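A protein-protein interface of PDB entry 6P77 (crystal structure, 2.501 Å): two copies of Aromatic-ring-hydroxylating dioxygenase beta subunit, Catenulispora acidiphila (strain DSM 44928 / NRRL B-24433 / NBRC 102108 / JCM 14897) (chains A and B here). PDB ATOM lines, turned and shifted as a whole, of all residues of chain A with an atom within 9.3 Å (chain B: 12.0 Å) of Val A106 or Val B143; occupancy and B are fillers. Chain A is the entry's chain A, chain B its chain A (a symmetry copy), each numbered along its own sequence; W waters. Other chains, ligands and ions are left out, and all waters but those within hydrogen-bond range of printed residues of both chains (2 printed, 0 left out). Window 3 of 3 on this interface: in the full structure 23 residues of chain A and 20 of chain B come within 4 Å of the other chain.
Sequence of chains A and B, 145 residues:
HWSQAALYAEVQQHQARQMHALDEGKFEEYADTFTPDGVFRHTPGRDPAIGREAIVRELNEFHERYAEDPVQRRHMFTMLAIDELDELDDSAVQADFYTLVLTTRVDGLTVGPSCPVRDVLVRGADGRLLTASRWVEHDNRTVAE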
ATOM      1  N   PRO A  70       7.790  10.927  16.909  1.00  0.00           N
ATOM      2  CA  PRO A  70       8.797  11.999  17.168  1.00  0.00           C
ATOM      3  C   PRO A  70       9.310  12.613  15.844  1.00  0.00           C
ATOM      4  O   PRO A  70      10.436  12.456  15.433  1.00  0.00           O
ATOM      5  CB  PRO A  70       9.899  11.313  17.989  1.00  0.00           C
ATOM      6  CG  PRO A  70       9.327   9.994  18.404  1.00  0.00           C
ATOM      7  CD  PRO A  70       8.197   9.628  17.457  1.00  0.00           C
ATOM      8  N   VAL A  71       8.422  13.372  15.215  1.00  0.00           N
ATOM      9  CA  VAL A  71       8.465  13.664  13.830  1.00  0.00           C
ATOM     10  C   VAL A  71       7.913  15.096  13.590  1.00  0.00           C
ATOM     11  O   VAL A  71       7.040  15.554  14.297  1.00  0.00           O
ATOM     12  CB  VAL A  71       7.601  12.609  13.109  1.00  0.00           C
ATOM     13  CG1 VAL A  71       6.178  12.664  13.608  1.00  0.00           C
ATOM     14  CG2 VAL A  71       7.526  12.823  11.612  1.00  0.00           C
ATOM     15  N   GLN A  72       8.464  15.779  12.580  1.00  0.00           N
ATOM     16  CA  GLN A  72       7.974  17.054  12.103  1.00  0.00           C
ATOM     17  C   GLN A  72       7.818  17.000  10.585  1.00  0.00           C
ATOM     18  O   GLN A  72       8.795  16.826   9.845  1.00  0.00           O
ATOM     19  CB  GLN A  72       8.942  18.184  12.481  1.00  0.00           C
ATOM     20  CG  GLN A  72       8.495  19.553  11.980  1.00  0.00           C
ATOM     21  CD  GLN A  72       7.196  19.964  12.604  1.00  0.00           C
ATOM     22  OE1 GLN A  72       7.131  20.039  13.828  1.00  0.00           O
ATOM     23  NE2 GLN A  72       6.135  20.188  11.783  1.00  0.00           N
ATOM     24  N   ARG A  73       6.575  17.168  10.133  1.00  0.00           N
ATOM     25  CA  ARG A  73       6.212  17.175   8.742  1.00  0.00           C
ATOM     26  C   ARG A  73       6.044  18.641   8.298  1.00  0.00           C
ATOM     27  O   ARG A  73       5.674  19.510   9.097  1.00  0.00           O
ATOM     28  CB  ARG A  73       4.952  16.302   8.550  1.00  0.00           C
ATOM     29  CG  ARG A  73       4.524  16.057   7.089  1.00  0.00           C
ATOM     30  CD  ARG A  73       3.782  14.737   6.791  1.00  0.00           C
ATOM     31  NE  ARG A  73       3.843  13.674   7.817  1.00  0.00           N
ATOM     32  CZ  ARG A  73       4.284  12.410   7.645  1.00  0.00           C
ATOM     33  NH1 ARG A  73       4.743  11.993   6.458  1.00  0.00           N
ATOM     34  NH2 ARG A  73       4.270  11.540   8.680  1.00  0.00           N
ATOM     35  N   ARG A  74       6.434  18.924   7.051  1.00  0.00           N
ATOM     36  CA  ARG A  74       6.186  20.208   6.388  1.00  0.00           C
ATOM     37  C   ARG A  74       5.617  19.914   5.003  1.00  0.00           C
ATOM     38  O   ARG A  74       6.136  19.056   4.285  1.00  0.00           O
ATOM     39  CB  ARG A  74       7.451  21.051   6.238  1.00  0.00           C
ATOM     40  CG  ARG A  74       8.110  21.488   7.517  1.00  0.00           C
ATOM     41  CD  ARG A  74       7.313  22.539   8.264  1.00  0.00           C
ATOM     42  NE  ARG A  74       7.834  22.690   9.629  1.00  0.00           N
ATOM     43  CZ  ARG A  74       7.176  23.185  10.676  1.00  0.00           C
ATOM     44  NH1 ARG A  74       5.933  23.605  10.576  1.00  0.00           N
ATOM     45  NH2 ARG A  74       7.782  23.273  11.838  1.00  0.00           N
ATOM     46  N   LEU A 102       7.784  16.963   3.284  1.00  0.00           N
ATOM     47  CA  LEU A 102       9.071  16.812   3.967  1.00  0.00           C
ATOM     48  C   LEU A 102       8.814  16.308   5.369  1.00  0.00           C
ATOM     49  O   LEU A 102       7.974  16.836   6.055  1.00  0.00           O
ATOM     50  CB  LEU A 102       9.808  18.127   4.073  1.00  0.00           C
ATOM     51  CG  LEU A 102      10.091  18.849   2.745  1.00  0.00           C
ATOM     52  CD1 LEU A 102      10.764  20.145   3.076  1.00  0.00           C
ATOM     53  CD2 LEU A 102      10.996  18.059   1.799  1.00  0.00           C
ATOM     54  N   THR A 103       9.568  15.286   5.795  1.00  0.00           N
ATOM     55  CA  THR A 103       9.407  14.741   7.117  1.00  0.00           C
ATOM     56  C   THR A 103      10.770  14.669   7.765  1.00  0.00           C
ATOM     57  O   THR A 103      11.629  14.022   7.257  1.00  0.00           O
ATOM     58  CB  THR A 103       8.769  13.346   7.058  1.00  0.00           C
ATOM     59  OG1 THR A 103       7.600  13.399   6.234  1.00  0.00           O
ATOM     60  CG2 THR A 103       8.428  12.840   8.451  1.00  0.00           C
ATOM     61  N   THR A 104      10.947  15.378   8.885  1.00  0.00           N
ATOM     62  CA  THR A 104      12.141  15.342   9.672  1.00  0.00           C
ATOM     63  C   THR A 104      11.883  14.399  10.854  1.00  0.00           C
ATOM     64  O   THR A 104      10.874  14.525  11.603  1.00  0.00           O
ATOM     65  CB  THR A 104      12.573  16.736  10.192  1.00  0.00           C
ATOM     66  OG1 THR A 104      12.871  17.601   9.098  1.00  0.00           O
ATOM     67  CG2 THR A 104      13.850  16.608  11.020  1.00  0.00           C
ATOM     68  N   ARG A 105      12.811  13.450  11.008  1.00  0.00           N
ATOM     69  CA  ARG A 105      12.844  12.521  12.109  1.00  0.00           C
ATOM     70  C   ARG A 105      14.227  12.534  12.703  1.00  0.00           C
ATOM     71  O   ARG A 105      15.149  13.091  12.116  1.00  0.00           O
ATOM     72  CB  ARG A 105      12.537  11.154  11.594  1.00  0.00           C
ATOM     73  CG  ARG A 105      11.084  10.919  11.320  1.00  0.00           C
ATOM     74  CD  ARG A 105      10.868   9.483  10.919  1.00  0.00           C
ATOM     75  NE  ARG A 105       9.553   9.309  10.321  1.00  0.00           N
ATOM     76  CZ  ARG A 105       9.283   9.488   9.026  1.00  0.00           C
ATOM     77  NH1 ARG A 105      10.246   9.831   8.162  1.00  0.00           N
ATOM     78  NH2 ARG A 105       8.042   9.290   8.592  1.00  0.00           N
ATOM     79  N   VAL A 106      14.383  11.885  13.852  1.00  0.00           N
ATOM     80  CA  VAL A 106      15.678  11.844  14.541  1.00  0.00           C
ATOM     81  C   VAL A 106      16.804  11.269  13.669  1.00  0.00           C
ATOM     82  O   VAL A 106      17.963  11.684  13.786  1.00  0.00           O
ATOM     83  CB  VAL A 106      15.609  11.076  15.874  1.00  0.00           C
ATOM     84  CG1 VAL A 106      15.140   9.636  15.669  1.00  0.00           C
ATOM     85  CG2 VAL A 106      16.969  11.084  16.564  1.00  0.00           C
ATOM     86  N   ASP A 107      16.462  10.317  12.795  1.00  0.00           N
ATOM     87  CA  ASP A 107      17.447   9.734  11.871  1.00  0.00           C
ATOM     88  C   ASP A 107      17.520  10.385  10.494  1.00  0.00           C
ATOM     89  O   ASP A 107      18.272   9.945   9.654  1.00  0.00           O
ATOM     90  CB  ASP A 107      17.214   8.249  11.694  1.00  0.00           C
ATOM     91  CG  ASP A 107      15.923   7.962  11.029  1.00  0.00           C
ATOM     92  OD1 ASP A 107      14.948   8.721  11.238  1.00  0.00           O
ATOM     93  OD2 ASP A 107      15.881   6.964  10.288  1.00  0.00           O
ATOM     94  N   GLY A 108      16.732  11.428  10.250  1.00  0.00           N
ATOM     95  CA  GLY A 108      16.993  12.263   9.098  1.00  0.00           C
ATOM     96  C   GLY A 108      15.775  12.854   8.479  1.00  0.00           C
ATOM     97  O   GLY A 108      14.721  12.799   9.053  1.00  0.00           O
ATOM     98  N   LEU A 109      15.938  13.403   7.281  1.00  0.00           N
ATOM     99  CA  LEU A 109      14.866  14.034   6.517  1.00  0.00           C
ATOM    100  C   LEU A 109      14.486  13.094   5.361  1.00  0.00           C
ATOM    101  O   LEU A 109      15.319  12.375   4.830  1.00  0.00           O
ATOM    102  CB  LEU A 109      15.344  15.359   5.972  1.00  0.00           C
ATOM    103  CG  LEU A 109      14.376  16.243   5.184  1.00  0.00           C
ATOM    104  CD1 LEU A 109      13.031  16.430   5.876  1.00  0.00           C
ATOM    105  CD2 LEU A 109      15.051  17.606   4.985  1.00  0.00           C
ATOM    106  N   THR A 110      13.196  13.014   5.073  1.00  0.00           N
ATOM    107  CA  THR A 110      12.651  12.238   4.006  1.00  0.00           C
ATOM    108  C   THR A 110      12.018  13.297   3.113  1.00  0.00           C
ATOM    109  O   THR A 110      11.401  14.295   3.604  1.00  0.00           O
ATOM    110  CB  THR A 110      11.583  11.231   4.521  1.00  0.00           C
ATOM    111  OG1 THR A 110      12.172   9.975   4.841  1.00  0.00           O
ATOM    112  CG2 THR A 110      10.648  10.905   3.470  1.00  0.00           C
ATOM    113  N   PRO B  44      19.451  28.368  15.905  1.00  0.00           N
ATOM    114  CA  PRO B  44      19.054  28.180  17.299  1.00  0.00           C
ATOM    115  C   PRO B  44      20.266  27.888  18.165  1.00  0.00           C
ATOM    116  O   PRO B  44      21.192  27.193  17.698  1.00  0.00           O
ATOM    117  CB  PRO B  44      18.171  26.934  17.244  1.00  0.00           C
ATOM    118  CG  PRO B  44      17.650  26.885  15.854  1.00  0.00           C
ATOM    119  CD  PRO B  44      18.676  27.533  14.973  1.00  0.00           C
ATOM    120  N   PRO B 113      18.385  21.473   6.044  1.00  0.00           N
ATOM    121  CA  PRO B 113      17.151  21.294   6.813  1.00  0.00           C
ATOM    122  C   PRO B 113      15.951  22.091   6.292  1.00  0.00           C
ATOM    123  O   PRO B 113      16.087  22.937   5.396  1.00  0.00           O
ATOM    124  CB  PRO B 113      17.545  21.870   8.181  1.00  0.00           C
ATOM    125  CG  PRO B 113      18.508  22.991   7.824  1.00  0.00           C
ATOM    126  CD  PRO B 113      19.333  22.383   6.706  1.00  0.00           C
ATOM    127  N   SER B 114      14.780  21.795   6.853  1.00  0.00           N
ATOM    128  CA  SER B 114      13.603  22.631   6.687  1.00  0.00           C
ATOM    129  C   SER B 114      13.526  23.500   7.928  1.00  0.00           C
ATOM    130  O   SER B 114      13.779  23.034   9.046  1.00  0.00           O
ATOM    131  CB  SER B 114      12.297  21.843   6.468  1.00  0.00           C
ATOM    132  OG  SER B 114      11.924  21.093   7.595  1.00  0.00           O
ATOM    133  N   CYS B 115      13.186  24.775   7.706  1.00  0.00           N
ATOM    134  CA  CYS B 115      13.214  25.809   8.712  1.00  0.00           C
ATOM    135  C   CYS B 115      11.973  26.701   8.670  1.00  0.00           C
ATOM    136  O   CYS B 115      11.772  27.484   7.736  1.00  0.00           O
ATOM    137  CB  CYS B 115      14.467  26.669   8.477  1.00  0.00           C
ATOM    138  SG  CYS B 115      16.046  25.769   8.497  1.00  0.00           S
ATOM    139  N   PRO B 116      11.087  26.628   9.678  1.00  0.00           N
ATOM    140  CA  PRO B 116      10.067  27.663   9.835  1.00  0.00           C
ATOM    141  C   PRO B 116      10.777  28.966  10.184  1.00  0.00           C
ATOM    142  O   PRO B 116      11.703  28.955  11.000  1.00  0.00           O
ATOM    143  CB  PRO B 116       9.210  27.177  11.013  1.00  0.00           C
ATOM    144  CG  PRO B 116       9.924  26.054  11.633  1.00  0.00           C
ATOM    145  CD  PRO B 116      11.044  25.590  10.715  1.00  0.00           C
ATOM    146  N   GLU B 137      14.019  29.052  12.859  1.00  0.00           N
ATOM    147  CA  GLU B 137      14.005  27.818  13.651  1.00  0.00           C
ATOM    148  C   GLU B 137      14.415  26.657  12.711  1.00  0.00           C
ATOM    149  O   GLU B 137      14.295  26.788  11.496  1.00  0.00           O
ATOM    150  CB  GLU B 137      12.644  27.621  14.320  1.00  0.00           C
ATOM    151  CG  GLU B 137      12.561  26.353  15.155  1.00  0.00           C
ATOM    152  CD  GLU B 137      13.635  26.286  16.237  1.00  0.00           C
ATOM    153  OE1 GLU B 137      13.665  27.214  17.083  1.00  0.00           O
ATOM    154  OE2 GLU B 137      14.445  25.322  16.233  1.00  0.00           O
ATOM    155  N   HIS B 138      14.990  25.579  13.271  1.00  0.00           N
ATOM    156  CA  HIS B 138      15.417  24.384  12.501  1.00  0.00           C
ATOM    157  C   HIS B 138      14.604  23.192  12.955  1.00  0.00           C
ATOM    158  O   HIS B 138      14.570  22.892  14.154  1.00  0.00           O
ATOM    159  CB  HIS B 138      16.907  24.057  12.746  1.00  0.00           C
ATOM    160  CG  HIS B 138      17.859  25.054  12.153  1.00  0.00           C
ATOM    161  ND1 HIS B 138      19.205  24.803  12.017  1.00  0.00           N
ATOM    162  CD2 HIS B 138      17.658  26.298  11.652  1.00  0.00           C
ATOM    163  CE1 HIS B 138      19.791  25.848  11.460  1.00  0.00           C
ATOM    164  NE2 HIS B 138      18.873  26.767  11.222  1.00  0.00           N
ATOM    165  N   ASP B 139      13.974  22.490  12.005  1.00  0.00           N
ATOM    166  CA  ASP B 139      13.112  21.353  12.351  1.00  0.00           C
ATOM    167  C   ASP B 139      13.851  20.176  12.955  1.00  0.00           C
ATOM    168  O   ASP B 139      13.264  19.438  13.754  1.00  0.00           O
ATOM    169  CB  ASP B 139      12.221  20.919  11.183  1.00  0.00           C
ATOM    170  CG  ASP B 139      11.053  21.902  10.925  1.00  0.00           C
ATOM    171  OD1 ASP B 139      10.571  22.582  11.866  1.00  0.00           O
ATOM    172  OD2 ASP B 139      10.588  21.961   9.779  1.00  0.00           O
ATOM    173  N   ASN B 140      15.134  20.005  12.600  1.00  0.00           N
ATOM    174  CA  ASN B 140      15.983  19.004  13.282  1.00  0.00           C
ATOM    175  C   ASN B 140      16.192  19.322  14.771  1.00  0.00           C
ATOM    176  O   ASN B 140      16.139  18.420  15.598  1.00  0.00           O
ATOM    177  CB  ASN B 140      17.281  18.589  12.527  1.00  0.00           C
ATOM    178  CG  ASN B 140      17.985  19.728  11.848  1.00  0.00           C
ATOM    179  OD1 ASN B 140      18.023  20.859  12.332  1.00  0.00           O
ATOM    180  ND2 ASN B 140      18.545  19.433  10.716  1.00  0.00           N
ATOM    181  N   ARG B 141      16.357  20.604  15.103  1.00  0.00           N
ATOM    182  CA  ARG B 141      16.495  21.032  16.501  1.00  0.00           C
ATOM    183  C   ARG B 141      15.217  20.751  17.280  1.00  0.00           C
ATOM    184  O   ARG B 141      15.264  20.230  18.383  1.00  0.00           O
ATOM    185  CB  ARG B 141      16.915  22.502  16.604  1.00  0.00           C
ATOM    186  CG  ARG B 141      17.080  23.017  18.033  1.00  0.00           C
ATOM    187  CD  ARG B 141      15.943  23.961  18.378  1.00  0.00           C
ATOM    188  NE  ARG B 141      16.174  24.629  19.647  1.00  0.00           N
ATOM    189  CZ  ARG B 141      15.762  25.860  19.968  1.00  0.00           C
ATOM    190  NH1 ARG B 141      15.075  26.609  19.108  1.00  0.00           N
ATOM    191  NH2 ARG B 141      16.061  26.340  21.177  1.00  0.00           N
ATOM    192  N   THR B 142      14.078  21.067  16.665  1.00  0.00           N
ATOM    193  CA  THR B 142      12.763  20.791  17.214  1.00  0.00           C
ATOM    194  C   THR B 142      12.545  19.310  17.487  1.00  0.00           C
ATOM    195  O   THR B 142      12.087  18.939  18.558  1.00  0.00           O
ATOM    196  CB  THR B 142      11.697  21.332  16.245  1.00  0.00           C
ATOM    197  OG1 THR B 142      11.756  22.760  16.300  1.00  0.00           O
ATOM    198  CG2 THR B 142      10.281  20.804  16.554  1.00  0.00           C
ATOM    199  N   VAL B 143      12.881  18.463  16.511  1.00  0.00           N
ATOM    200  CA  VAL B 143      12.732  17.025  16.657  1.00  0.00           C
ATOM    201  C   VAL B 143      13.662  16.551  17.772  1.00  0.00           C
ATOM    202  O   VAL B 143      13.229  15.808  18.644  1.00  0.00           O
ATOM    203  CB  VAL B 143      12.914  16.305  15.302  1.00  0.00           C
ATOM    204  CG1 VAL B 143      13.105  14.813  15.441  1.00  0.00           C
ATOM    205  CG2 VAL B 143      11.700  16.561  14.439  1.00  0.00           C
ATOM    206  N   ALA B 144      14.915  17.026  17.773  1.00  0.00           N
ATOM    207  CA  ALA B 144      15.879  16.712  18.849  1.00  0.00           C
ATOM    208  C   ALA B 144      15.354  16.972  20.310  1.00  0.00           C
ATOM    209  O   ALA B 144      15.177  18.123  20.765  1.00  0.00           O
ATOM    210  CB  ALA B 144      17.203  17.420  18.591  1.00  0.00           C
ATOM    211  N   GLU B 145      15.105  15.857  21.012  1.00  0.00           N
ATOM    212  CA  GLU B 145      14.490  15.783  22.357  1.00  0.00           C
ATOM    213  C   GLU B 145      14.361  14.326  22.880  1.00  0.00           C
ATOM    214  O   GLU B 145      14.064  13.396  22.126  1.00  0.00           O
ATOM    215  CB  GLU B 145      13.102  16.417  22.375  1.00  0.00           C
ATOM    216  CG  GLU B 145      12.038  15.485  21.821  1.00  0.00           C
ATOM    217  CD  GLU B 145      10.833  16.231  21.313  1.00  0.00           C
ATOM    218  OE1 GLU B 145      10.967  17.399  20.902  1.00  0.00           O
ATOM    219  OE2 GLU B 145       9.750  15.630  21.317  1.00  0.00           O
ATOM    220  OXT GLU B 145      14.519  14.034  24.071  1.00  0.00           O
HETATM  221  O   HOH W   1      10.549  18.804   8.325  1.00  0.00           O
HETATM  222  O   HOH W   2      14.943  19.678   8.788  1.00  0.00           O
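Of the 14 printed residues of chain A, 6 touch a printed residue of chain B.
Of the 14 printed residues of chain B, 5 touch a printed residue of chain A.
Printed residues of chain B that touch a printed residue of chain A: Ser B114, Pro B116, Asp B139, Asn B140 and Val B143.
Among the printed residues, 12 pairs touch across the chains.
Among the printed residues, Asp or Glu carboxylates within 4 Å of a Lys or Arg side-chain nitrogen of the other chain: Arg A74 with Asp B139.
The backbone carbonyl oxygen of Pro B116 is in hydrogen-bond range of the backbone NH of Glu B137, at 3.0 Å.
O of Gln A72 lies within hydrogen-bond range of N of Thr A104 (2.8 Å).
The side-chain hydroxyl of Ser B114 lies within hydrogen-bond range of the side-chain carboxylate of Asp B139, 2.7 Å away.
The side-chain amide nitrogen (NE2) of Gln A72 lies close to the guanidinium group (NH2) of Arg A74 (3.5 Å).
The backbone carbonyl oxygen of Leu A102 lies within hydrogen-bond range of the backbone NH of Arg A74 (2.8 Å).
Water W1 lies within hydrogen-bond range of OG1 of Thr A104 (2.7 Å), OG of Ser B114 (2.8 Å), O of Gln A72 (3.0 Å) and OD2 of Asp B139 (3.5 Å).
Water W2 lies within hydrogen-bond range of the backbone NH (N) of Ser B114 and the side-chain hydroxyl (OG1) of Thr A104.
No position is printed for both chains.
Of the 12 pairs that touch across the chains among the printed residues, none has its exchanged pair printed and touching as well.
Val A106 touches one residue of chain B.
Val B143 touches just these residues of chain A: Pro A70 (3.6 Å), Gln A72 (3.8 Å), Thr A104 (3.6 Å), Arg A105 (3.7 Å) and Val A106 (3.6 Å).
No residue of chain B comes within 4 Å of Asp A107.
No residue of chain B comes within 4 Å of Gly A108.
No residue of chain A comes within 4 Å of Thr B142.
No residue of chain A comes within 4 Å of Ala B144.
Printed residues of chain A within 4 Å of Ser B114: Arg A74 (3.8 Å) and Thr A104 (3.9 Å).
Of the printed residues of chain A, Asp B139 touches Gln A72, Arg A74 and Thr A104.
Leu A102 touches none of the printed residues of chain B.
NE of Arg A74 lies within salt-bridge range of OD2 of Asp B139 (2.9 Å).
O of Pro A70 touches CG1 of Val B143, 3.6 Å away.
CG of Gln A72 touches CG of Asp B139, at 3.6 Å.
Gln A72 touches Val B143 (CB to CG2, 3.8 Å).
Arg A74 touches Ser B114.
Pro B116 touches Arg A74.
Thr A104 touches Ser B114.
Thr A104 touches Asp B139 (OG1 to CB, 3.97 Å).
Asn B140 touches Thr A104 (CA to CG2, 3.9 Å).
Val B143 touches Thr A104 (CG2 to O, 3.6 Å).
N of Val A106 touches CG1 of Val B143, at 3.6 Å.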
